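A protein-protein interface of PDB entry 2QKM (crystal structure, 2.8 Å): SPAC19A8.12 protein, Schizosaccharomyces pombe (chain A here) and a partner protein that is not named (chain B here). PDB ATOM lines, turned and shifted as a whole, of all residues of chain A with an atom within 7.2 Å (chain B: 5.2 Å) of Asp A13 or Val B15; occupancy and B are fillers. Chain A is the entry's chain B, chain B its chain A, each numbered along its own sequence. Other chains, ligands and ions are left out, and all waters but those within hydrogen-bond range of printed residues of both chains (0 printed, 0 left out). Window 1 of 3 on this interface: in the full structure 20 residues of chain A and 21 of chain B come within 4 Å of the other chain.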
ATOM      1  N   PHE A   3      18.797   2.362 -16.664  1.00  0.00           N
ATOM      2  CA  PHE A   3      19.926   1.455 -16.925  1.00  0.00           C
ATOM      3  C   PHE A   3      21.008   1.406 -15.839  1.00  0.00           C
ATOM      4  O   PHE A   3      22.084   0.847 -16.078  1.00  0.00           O
ATOM      5  CB  PHE A   3      20.622   1.810 -18.241  1.00  0.00           C
ATOM      6  CG  PHE A   3      19.736   1.757 -19.439  1.00  0.00           C
ATOM      7  CD1 PHE A   3      19.324   2.937 -20.062  1.00  0.00           C
ATOM      8  CD2 PHE A   3      19.326   0.537 -19.965  1.00  0.00           C
ATOM      9  CE1 PHE A   3      18.506   2.902 -21.182  1.00  0.00           C
ATOM     10  CE2 PHE A   3      18.506   0.484 -21.082  1.00  0.00           C
ATOM     11  CZ  PHE A   3      18.099   1.665 -21.698  1.00  0.00           C
ATOM     12  N   THR A   7      22.587  -5.121 -16.490  1.00  0.00           N
ATOM     13  CA  THR A   7      23.875  -5.690 -16.819  1.00  0.00           C
ATOM     14  C   THR A   7      24.329  -5.155 -18.187  1.00  0.00           C
ATOM     15  O   THR A   7      23.616  -4.374 -18.822  1.00  0.00           O
ATOM     16  CB  THR A   7      23.808  -7.214 -16.856  1.00  0.00           C
ATOM     17  OG1 THR A   7      22.842  -7.609 -17.827  1.00  0.00           O
ATOM     18  CG2 THR A   7      23.397  -7.777 -15.522  1.00  0.00           C
ATOM     19  N   PHE A   8      25.520  -5.547 -18.641  1.00  0.00           N
ATOM     20  CA  PHE A   8      25.982  -5.137 -19.963  1.00  0.00           C
ATOM     21  C   PHE A   8      25.116  -5.817 -21.023  1.00  0.00           C
ATOM     22  O   PHE A   8      24.775  -5.226 -22.058  1.00  0.00           O
ATOM     23  CB  PHE A   8      27.457  -5.471 -20.149  1.00  0.00           C
ATOM     24  CG  PHE A   8      28.049  -4.972 -21.445  1.00  0.00           C
ATOM     25  CD1 PHE A   8      27.624  -3.776 -22.023  1.00  0.00           C
ATOM     26  CD2 PHE A   8      29.079  -5.673 -22.063  1.00  0.00           C
ATOM     27  CE1 PHE A   8      28.185  -3.300 -23.223  1.00  0.00           C
ATOM     28  CE2 PHE A   8      29.660  -5.208 -23.265  1.00  0.00           C
ATOM     29  CZ  PHE A   8      29.211  -4.013 -23.846  1.00  0.00           C
ATOM     30  N   SER A   9      24.760  -7.061 -20.728  1.00  0.00           N
ATOM     31  CA  SER A   9      23.982  -7.902 -21.595  1.00  0.00           C
ATOM     32  C   SER A   9      22.554  -7.323 -21.813  1.00  0.00           C
ATOM     33  O   SER A   9      22.067  -7.258 -22.964  1.00  0.00           O
ATOM     34  CB  SER A   9      23.970  -9.298 -20.987  1.00  0.00           C
ATOM     35  OG  SER A   9      23.071 -10.149 -21.650  1.00  0.00           O
ATOM     36  N   GLN A  10      21.908  -6.886 -20.723  1.00  0.00           N
ATOM     37  CA  GLN A  10      20.593  -6.250 -20.781  1.00  0.00           C
ATOM     38  C   GLN A  10      20.641  -4.911 -21.543  1.00  0.00           C
ATOM     39  O   GLN A  10      19.711  -4.562 -22.280  1.00  0.00           O
ATOM     40  CB  GLN A  10      20.026  -6.032 -19.371  1.00  0.00           C
ATOM     41  CG  GLN A  10      19.632  -7.299 -18.645  1.00  0.00           C
ATOM     42  CD  GLN A  10      19.037  -7.059 -17.249  1.00  0.00           C
ATOM     43  OE1 GLN A  10      17.937  -7.548 -16.945  1.00  0.00           O
ATOM     44  NE2 GLN A  10      19.764  -6.324 -16.388  1.00  0.00           N
ATOM     45  N   VAL A  11      21.709  -4.155 -21.340  1.00  0.00           N
ATOM     46  CA  VAL A  11      21.936  -2.931 -22.077  1.00  0.00           C
ATOM     47  C   VAL A  11      22.109  -3.247 -23.565  1.00  0.00           C
ATOM     48  O   VAL A  11      21.604  -2.520 -24.428  1.00  0.00           O
ATOM     49  CB  VAL A  11      23.186  -2.183 -21.553  1.00  0.00           C
ATOM     50  CG1 VAL A  11      23.717  -1.223 -22.598  1.00  0.00           C
ATOM     51  CG2 VAL A  11      22.877  -1.466 -20.226  1.00  0.00           C
ATOM     52  N   LEU A  12      22.794  -4.336 -23.880  1.00  0.00           N
ATOM     53  CA  LEU A  12      22.978  -4.666 -25.281  1.00  0.00           C
ATOM     54  C   LEU A  12      21.667  -5.069 -25.964  1.00  0.00           C
ATOM     55  O   LEU A  12      21.468  -4.793 -27.135  1.00  0.00           O
ATOM     56  CB  LEU A  12      24.092  -5.705 -25.469  1.00  0.00           C
ATOM     57  CG  LEU A  12      25.512  -5.108 -25.337  1.00  0.00           C
ATOM     58  CD1 LEU A  12      26.549  -6.202 -25.161  1.00  0.00           C
ATOM     59  CD2 LEU A  12      25.897  -4.194 -26.505  1.00  0.00           C
ATOM     60  N   ASP A  13      20.767  -5.704 -25.228  1.00  0.00           N
ATOM     61  CA  ASP A  13      19.496  -6.149 -25.797  1.00  0.00           C
ATOM     62  C   ASP A  13      18.614  -4.955 -26.109  1.00  0.00           C
ATOM     63  O   ASP A  13      17.975  -4.891 -27.175  1.00  0.00           O
ATOM     64  CB  ASP A  13      18.763  -7.077 -24.829  1.00  0.00           C
ATOM     65  CG  ASP A  13      19.300  -8.503 -24.848  1.00  0.00           C
ATOM     66  OD1 ASP A  13      20.059  -8.883 -25.765  1.00  0.00           O
ATOM     67  OD2 ASP A  13      18.929  -9.264 -23.937  1.00  0.00           O
ATOM     68  N   ASP A  14      18.594  -4.013 -25.164  1.00  0.00           N
ATOM     69  CA  ASP A  14      17.814  -2.797 -25.275  1.00  0.00           C
ATOM     70  C   ASP A  14      18.189  -2.009 -26.521  1.00  0.00           C
ATOM     71  O   ASP A  14      17.350  -1.687 -27.365  1.00  0.00           O
ATOM     72  CB  ASP A  14      18.046  -1.922 -24.051  1.00  0.00           C
ATOM     73  CG  ASP A  14      17.264  -0.638 -24.120  1.00  0.00           C
ATOM     74  OD1 ASP A  14      16.150  -0.576 -23.553  1.00  0.00           O
ATOM     75  OD2 ASP A  14      17.763   0.294 -24.784  1.00  0.00           O
ATOM     76  N   LEU A  15      19.467  -1.683 -26.603  1.00  0.00           N
ATOM     77  CA  LEU A  15      19.999  -0.956 -27.743  1.00  0.00           C
ATOM     78  C   LEU A  15      19.655  -1.676 -29.034  1.00  0.00           C
ATOM     79  O   LEU A  15      19.384  -1.024 -30.048  1.00  0.00           O
ATOM     80  CB  LEU A  15      21.513  -0.756 -27.598  1.00  0.00           C
ATOM     81  CG  LEU A  15      21.887   0.274 -26.532  1.00  0.00           C
ATOM     82  CD1 LEU A  15      23.394   0.344 -26.319  1.00  0.00           C
ATOM     83  CD2 LEU A  15      21.334   1.631 -26.945  1.00  0.00           C
ATOM     84  N   SER A  16      19.632  -3.008 -28.991  1.00  0.00           N
ATOM     85  CA  SER A  16      19.282  -3.788 -30.170  1.00  0.00           C
ATOM     86  C   SER A  16      17.804  -3.609 -30.499  1.00  0.00           C
ATOM     87  O   SER A  16      17.462  -3.141 -31.572  1.00  0.00           O
ATOM     88  CB  SER A  16      19.629  -5.257 -29.966  1.00  0.00           C
ATOM     89  OG  SER A  16      19.191  -6.049 -31.044  1.00  0.00           O
ATOM     90  N   ALA A  17      16.936  -3.957 -29.552  1.00  0.00           N
ATOM     91  CA  ALA A  17      15.498  -3.785 -29.685  1.00  0.00           C
ATOM     92  C   ALA A  17      15.151  -2.371 -30.081  1.00  0.00           C
ATOM     93  O   ALA A  17      14.173  -2.149 -30.798  1.00  0.00           O
ATOM     94  CB  ALA A  17      14.832  -4.130 -28.395  1.00  0.00           C
ATOM     95  N   ARG A  18      15.961  -1.424 -29.611  1.00  0.00           N
ATOM     96  CA  ARG A  18      15.749   0.004 -29.832  1.00  0.00           C
ATOM     97  C   ARG A  18      16.115   0.448 -31.238  1.00  0.00           C
ATOM     98  O   ARG A  18      15.329   1.140 -31.871  1.00  0.00           O
ATOM     99  CB  ARG A  18      16.592   0.792 -28.841  1.00  0.00           C
ATOM    100  CG  ARG A  18      16.234   2.260 -28.620  1.00  0.00           C
ATOM    101  CD  ARG A  18      17.006   2.780 -27.397  1.00  0.00           C
ATOM    102  NE  ARG A  18      16.141   3.622 -26.595  1.00  0.00           N
ATOM    103  CZ  ARG A  18      15.472   3.234 -25.513  1.00  0.00           C
ATOM    104  NH1 ARG A  18      15.581   2.003 -25.041  1.00  0.00           N
ATOM    105  NH2 ARG A  18      14.687   4.104 -24.900  1.00  0.00           N
ATOM    106  N   PHE A  19      17.286   0.044 -31.736  1.00  0.00           N
ATOM    107  CA  PHE A  19      17.821   0.600 -32.988  1.00  0.00           C
ATOM    108  C   PHE A  19      17.828  -0.297 -34.239  1.00  0.00           C
ATOM    109  O   PHE A  19      17.469   0.168 -35.340  1.00  0.00           O
ATOM    110  CB  PHE A  19      19.214   1.153 -32.756  1.00  0.00           C
ATOM    111  CG  PHE A  19      19.243   2.379 -31.903  1.00  0.00           C
ATOM    112  CD1 PHE A  19      19.106   3.646 -32.476  1.00  0.00           C
ATOM    113  CD2 PHE A  19      19.420   2.285 -30.524  1.00  0.00           C
ATOM    114  CE1 PHE A  19      19.144   4.785 -31.690  1.00  0.00           C
ATOM    115  CE2 PHE A  19      19.451   3.424 -29.734  1.00  0.00           C
ATOM    116  CZ  PHE A  19      19.317   4.666 -30.321  1.00  0.00           C
ATOM    117  N   LEU A  21      17.300  -4.328 -34.160  1.00  0.00           N
ATOM    118  CA  LEU A  21      16.500  -5.558 -34.110  1.00  0.00           C
ATOM    119  C   LEU A  21      15.172  -5.565 -34.903  1.00  0.00           C
ATOM    120  O   LEU A  21      14.834  -6.550 -35.540  1.00  0.00           O
ATOM    121  CB  LEU A  21      16.236  -5.957 -32.653  1.00  0.00           C
ATOM    122  CG  LEU A  21      15.549  -7.302 -32.392  1.00  0.00           C
ATOM    123  CD1 LEU A  21      16.209  -8.429 -33.170  1.00  0.00           C
ATOM    124  CD2 LEU A  21      15.555  -7.625 -30.904  1.00  0.00           C
ATOM    125  N   LYS A  67      29.569  -6.283 -30.588  1.00  0.00           N
ATOM    126  CA  LYS A  67      28.774  -6.753 -29.454  1.00  0.00           C
ATOM    127  C   LYS A  67      27.279  -6.507 -29.665  1.00  0.00           C
ATOM    128  O   LYS A  67      26.434  -7.181 -29.082  1.00  0.00           O
ATOM    129  CB  LYS A  67      29.262  -6.122 -28.149  1.00  0.00           C
ATOM    130  CG  LYS A  67      30.498  -6.805 -27.569  1.00  0.00           C
ATOM    131  CD  LYS A  67      30.225  -7.508 -26.242  1.00  0.00           C
ATOM    132  CE  LYS A  67      29.425  -8.786 -26.348  1.00  0.00           C
ATOM    133  NZ  LYS A  67      30.148  -9.972 -26.898  1.00  0.00           N
ATOM    134  N   LEU A  68      26.939  -5.540 -30.505  1.00  0.00           N
ATOM    135  CA  LEU A  68      25.525  -5.309 -30.778  1.00  0.00           C
ATOM    136  C   LEU A  68      25.000  -6.405 -31.703  1.00  0.00           C
ATOM    137  O   LEU A  68      23.837  -6.762 -31.621  1.00  0.00           O
ATOM    138  CB  LEU A  68      25.251  -3.888 -31.309  1.00  0.00           C
ATOM    139  CG  LEU A  68      23.790  -3.439 -31.122  1.00  0.00           C
ATOM    140  CD1 LEU A  68      23.359  -3.479 -29.643  1.00  0.00           C
ATOM    141  CD2 LEU A  68      23.505  -2.063 -31.721  1.00  0.00           C
ATOM    142  N   ALA A  70      25.895  -9.586 -31.509  1.00  0.00           N
ATOM    143  CA  ALA A  70      25.631 -10.712 -30.627  1.00  0.00           C
ATOM    144  C   ALA A  70      24.218 -10.664 -30.037  1.00  0.00           C
ATOM    145  O   ALA A  70      23.682 -11.696 -29.635  1.00  0.00           O
ATOM    146  CB  ALA A  70      26.668 -10.782 -29.538  1.00  0.00           C
ATOM    147  N   HIS A  71      23.602  -9.487 -29.998  1.00  0.00           N
ATOM    148  CA  HIS A  71      22.249  -9.406 -29.463  1.00  0.00           C
ATOM    149  C   HIS A  71      21.206  -9.132 -30.548  1.00  0.00           C
ATOM    150  O   HIS A  71      20.110  -8.615 -30.267  1.00  0.00           O
ATOM    151  CB  HIS A  71      22.168  -8.408 -28.314  1.00  0.00           C
ATOM    152  CG  HIS A  71      23.058  -8.753 -27.161  1.00  0.00           C
ATOM    153  ND1 HIS A  71      22.569  -9.125 -25.926  1.00  0.00           N
ATOM    154  CD2 HIS A  71      24.410  -8.786 -27.053  1.00  0.00           C
ATOM    155  CE1 HIS A  71      23.579  -9.369 -25.109  1.00  0.00           C
ATOM    156  NE2 HIS A  71      24.708  -9.169 -25.769  1.00  0.00           N
ATOM    157  N   CYS A  72      21.537  -9.522 -31.781  1.00  0.00           N
ATOM    158  CA  CYS A  72      20.652  -9.316 -32.924  1.00  0.00           C
ATOM    159  C   CYS A  72      20.523 -10.538 -33.843  1.00  0.00           C
ATOM    160  O   CYS A  72      21.244 -10.643 -34.831  1.00  0.00           O
ATOM    161  CB  CYS A  72      21.130  -8.112 -33.724  1.00  0.00           C
ATOM    162  SG  CYS A  72      19.919  -7.621 -34.938  1.00  0.00           S
ATOM    163  N   ALA B  10      11.503 -13.019 -28.084  1.00  0.00           N
ATOM    164  CA  ALA B  10      11.985 -13.144 -26.708  1.00  0.00           C
ATOM    165  C   ALA B  10      12.831 -11.949 -26.248  1.00  0.00           C
ATOM    166  O   ALA B  10      12.692 -11.483 -25.107  1.00  0.00           O
ATOM    167  CB  ALA B  10      12.752 -14.438 -26.546  1.00  0.00           C
ATOM    168  N   VAL B  11      13.699 -11.450 -27.132  1.00  0.00           N
ATOM    169  CA  VAL B  11      14.519 -10.281 -26.814  1.00  0.00           C
ATOM    170  C   VAL B  11      13.605  -9.080 -26.629  1.00  0.00           C
ATOM    171  O   VAL B  11      13.722  -8.345 -25.648  1.00  0.00           O
ATOM    172  CB  VAL B  11      15.622  -9.984 -27.873  1.00  0.00           C
ATOM    173  CG1 VAL B  11      16.478  -8.850 -27.411  1.00  0.00           C
ATOM    174  CG2 VAL B  11      16.529 -11.180 -28.081  1.00  0.00           C
ATOM    175  N   ASN B  12      12.662  -8.908 -27.547  1.00  0.00           N
ATOM    176  CA  ASN B  12      11.755  -7.778 -27.479  1.00  0.00           C
ATOM    177  C   ASN B  12      11.018  -7.724 -26.174  1.00  0.00           C
ATOM    178  O   ASN B  12      10.990  -6.675 -25.525  1.00  0.00           O
ATOM    179  CB  ASN B  12      10.786  -7.793 -28.639  1.00  0.00           C
ATOM    180  CG  ASN B  12      11.411  -7.262 -29.898  1.00  0.00           C
ATOM    181  OD1 ASN B  12      12.385  -6.506 -29.850  1.00  0.00           O
ATOM    182  ND2 ASN B  12      10.866  -7.654 -31.036  1.00  0.00           N
ATOM    183  N   LEU B  13      10.474  -8.872 -25.779  1.00  0.00           N
ATOM    184  CA  LEU B  13       9.656  -9.001 -24.582  1.00  0.00           C
ATOM    185  C   LEU B  13      10.481  -8.786 -23.300  1.00  0.00           C
ATOM    186  O   LEU B  13       9.978  -8.218 -22.322  1.00  0.00           O
ATOM    187  CB  LEU B  13       8.919 -10.352 -24.580  1.00  0.00           C
ATOM    188  CG  LEU B  13       7.856 -10.569 -23.488  1.00  0.00           C
ATOM    189  CD1 LEU B  13       6.829  -9.437 -23.487  1.00  0.00           C
ATOM    190  CD2 LEU B  13       7.173 -11.928 -23.596  1.00  0.00           C
ATOM    191  N   GLN B  14      11.732  -9.239 -23.316  1.00  0.00           N
ATOM    192  CA  GLN B  14      12.666  -8.999 -22.210  1.00  0.00           C
ATOM    193  C   GLN B  14      12.909  -7.513 -22.073  1.00  0.00           C
ATOM    194  O   GLN B  14      12.820  -6.951 -20.975  1.00  0.00           O
ATOM    195  CB  GLN B  14      14.012  -9.658 -22.488  1.00  0.00           C
ATOM    196  CG  GLN B  14      14.285 -10.885 -21.714  1.00  0.00           C
ATOM    197  CD  GLN B  14      15.405 -11.694 -22.334  1.00  0.00           C
ATOM    198  OE1 GLN B  14      16.548 -11.227 -22.429  1.00  0.00           O
ATOM    199  NE2 GLN B  14      15.082 -12.921 -22.775  1.00  0.00           N
ATOM    200  N   VAL B  15      13.251  -6.890 -23.199  1.00  0.00           N
ATOM    201  CA  VAL B  15      13.592  -5.476 -23.218  1.00  0.00           C
ATOM    202  C   VAL B  15      12.458  -4.661 -22.587  1.00  0.00           C
ATOM    203  O   VAL B  15      12.713  -3.854 -21.700  1.00  0.00           O
ATOM    204  CB  VAL B  15      13.963  -4.998 -24.647  1.00  0.00           C
ATOM    205  CG1 VAL B  15      13.913  -3.498 -24.754  1.00  0.00           C
ATOM    206  CG2 VAL B  15      15.358  -5.486 -24.999  1.00  0.00           C
ATOM    207  N   LEU B  16      11.218  -4.929 -23.007  1.00  0.00           N
ATOM    208  CA  LEU B  16      10.044  -4.214 -22.512  1.00  0.00           C
ATOM    209  C   LEU B  16       9.704  -4.500 -21.044  1.00  0.00           C
ATOM    210  O   LEU B  16       9.561  -3.564 -20.247  1.00  0.00           O
ATOM    211  CB  LEU B  16       8.835  -4.497 -23.393  1.00  0.00           C
ATOM    212  CG  LEU B  16       8.903  -4.141 -24.880  1.00  0.00           C
ATOM    213  CD1 LEU B  16       7.534  -4.380 -25.442  1.00  0.00           C
ATOM    214  CD2 LEU B  16       9.352  -2.690 -25.136  1.00  0.00           C
ATOM    215  N   LYS B  17       9.575  -5.779 -20.694  1.00  0.00           N
ATOM    216  CA  LYS B  17       9.428  -6.193 -19.297  1.00  0.00           C
ATOM    217  C   LYS B  17      10.516  -5.616 -18.380  1.00  0.00           C
ATOM    218  O   LYS B  17      10.267  -5.351 -17.199  1.00  0.00           O
ATOM    219  CB  LYS B  17       9.418  -7.714 -19.184  1.00  0.00           C
ATOM    220  CG  LYS B  17       8.075  -8.376 -19.469  1.00  0.00           C
ATOM    221  CD  LYS B  17       8.073  -9.806 -18.959  1.00  0.00           C
ATOM    222  CE  LYS B  17       6.728 -10.460 -19.144  1.00  0.00           C
ATOM    223  NZ  LYS B  17       5.840 -10.305 -17.934  1.00  0.00           N
ATOM    224  N   PHE B  18      11.719  -5.419 -18.912  1.00  0.00           N
ATOM    225  CA  PHE B  18      12.775  -4.797 -18.116  1.00  0.00           C
ATOM    226  C   PHE B  18      12.408  -3.360 -17.760  1.00  0.00           C
ATOM    227  O   PHE B  18      12.721  -2.881 -16.678  1.00  0.00           O
ATOM    228  CB  PHE B  18      14.134  -4.824 -18.827  1.00  0.00           C
ATOM    229  CG  PHE B  18      15.220  -4.111 -18.064  1.00  0.00           C
ATOM    230  CD1 PHE B  18      15.876  -4.744 -17.001  1.00  0.00           C
ATOM    231  CD2 PHE B  18      15.564  -2.795 -18.378  1.00  0.00           C
ATOM    232  CE1 PHE B  18      16.863  -4.085 -16.275  1.00  0.00           C
ATOM    233  CE2 PHE B  18      16.559  -2.127 -17.655  1.00  0.00           C
ATOM    234  CZ  PHE B  18      17.202  -2.777 -16.602  1.00  0.00           C
ATOM    235  N   HIS B  19      11.757  -2.677 -18.695  1.00  0.00           N
ATOM    236  CA  HIS B  19      11.312  -1.308 -18.484  1.00  0.00           C
ATOM    237  C   HIS B  19       9.972  -1.299 -17.781  1.00  0.00           C
ATOM    238  O   HIS B  19       9.728  -0.436 -16.947  1.00  0.00           O
ATOM    239  CB  HIS B  19      11.225  -0.563 -19.820  1.00  0.00           C
ATOM    240  CG  HIS B  19      12.562  -0.326 -20.453  1.00  0.00           C
ATOM    241  ND1 HIS B  19      13.532   0.459 -19.865  1.00  0.00           N
ATOM    242  CD2 HIS B  19      13.096  -0.785 -21.607  1.00  0.00           C
ATOM    243  CE1 HIS B  19      14.605   0.472 -20.634  1.00  0.00           C
ATOM    244  NE2 HIS B  19      14.367  -0.275 -21.694  1.00  0.00           N
ATOM    245  N   LEU B  69      10.152   2.884 -27.577  1.00  0.00           N
ATOM    246  CA  LEU B  69      11.514   2.972 -27.071  1.00  0.00           C
ATOM    247  C   LEU B  69      12.239   4.067 -27.852  1.00  0.00           C
ATOM    248  O   LEU B  69      12.788   3.840 -28.939  1.00  0.00           O
ATOM    249  CB  LEU B  69      12.245   1.634 -27.164  1.00  0.00           C
ATOM    250  CG  LEU B  69      11.693   0.501 -26.309  1.00  0.00           C
ATOM    251  CD1 LEU B  69      12.492  -0.779 -26.568  1.00  0.00           C
ATOM    252  CD2 LEU B  69      11.676   0.860 -24.818  1.00  0.00           C
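OD2 of Asp A13 lies close to OE1 of Gln B14, at 3.4 Å.
The side-chain carboxylate of Asp A14 is in hydrogen-bond range of a ring nitrogen (NE2) of His B19.
Of chain B, only Val B11 (3.8 Å), Gln B14 (3.4 Å) and Val B15 (3.5 Å) come within 4 Å of Asp A13.
Val B15 touches three residues of chain A.
Of the printed residues of chain A, Leu B69 touches Arg A18 (3.8 Å).
Printed residues of chain A within 4 Å of Gln B14: Asp A13.
Of the printed residues of chain B, Arg A18 touches Leu B69 (3.8 Å).
Printed residues of chain B within 4 Å of Phe A3: His B19 (3.8 Å).
Phe A19 touches none of the printed residues of chain B.
The nearest printed residue of chain B that does not touch Asp A13 is Asn B12 (6.4 Å).
The nearest residue of chain A that does not touch Val B15 is Gln A10 (5.2 Å).
The nearest printed residue of chain B that does not touch Ala A17 is Leu B69 (4.5 Å).
Along chain B the printed residues that touch a printed residue of chain A span positions 11 to 69.
Hydrophobic or aromatic side chains of chain A within 4 Å of the printed part of chain B: Phe A3, Ala A17 and Leu A21.
Among the printed residues, 12 pairs touch across the chains.
Among the printed residues, no Asp or Glu carboxylate lies within 4 Å of a Lys or Arg side-chain nitrogen of the other chain.
CE1 of His B19 touches CZ of Phe A3, at 3.8 Å.
Gln A10 touches Phe B18 (OE1 to CD1, 3.5 Å).
Asp A13 touches Val B11.
Val B15 touches Asp A13 (CG2 to O, 3.5 Å).
N of Asp A14 touches CG2 of Val B15, at 3.6 Å.
Asn B12 touches Ala A17 (OD1 to CB, 3.7 Å).
CG2 of Val B15 touches CB of Ala A17 (3.7 Å).
Leu B69 touches Arg A18 (O to CG, 3.8 Å).
CG1 of Val B11 touches CD2 of Leu A21, 3.8 Å away.
Asn B12 touches Leu A21 (OD1 to CD2, 3.5 Å).
The backbone NH (N) of Thr A7 lies close to the side-chain amide nitrogen (NE2) of Gln A10 (3.1 Å).
The side-chain carboxylate (OD1) of Asp A13 lies within hydrogen-bond range of a ring nitrogen (ND1) of His A71 (2.5 Å).
The side-chain carboxylate (OD2) of Asp A14 is in salt-bridge range of the guanidinium group (NH1) of Arg A18.
The backbone NH of Leu A21 sits at hydrogen-bond distance from the backbone carbonyl oxygen of Ser A16 (2.9 Å).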
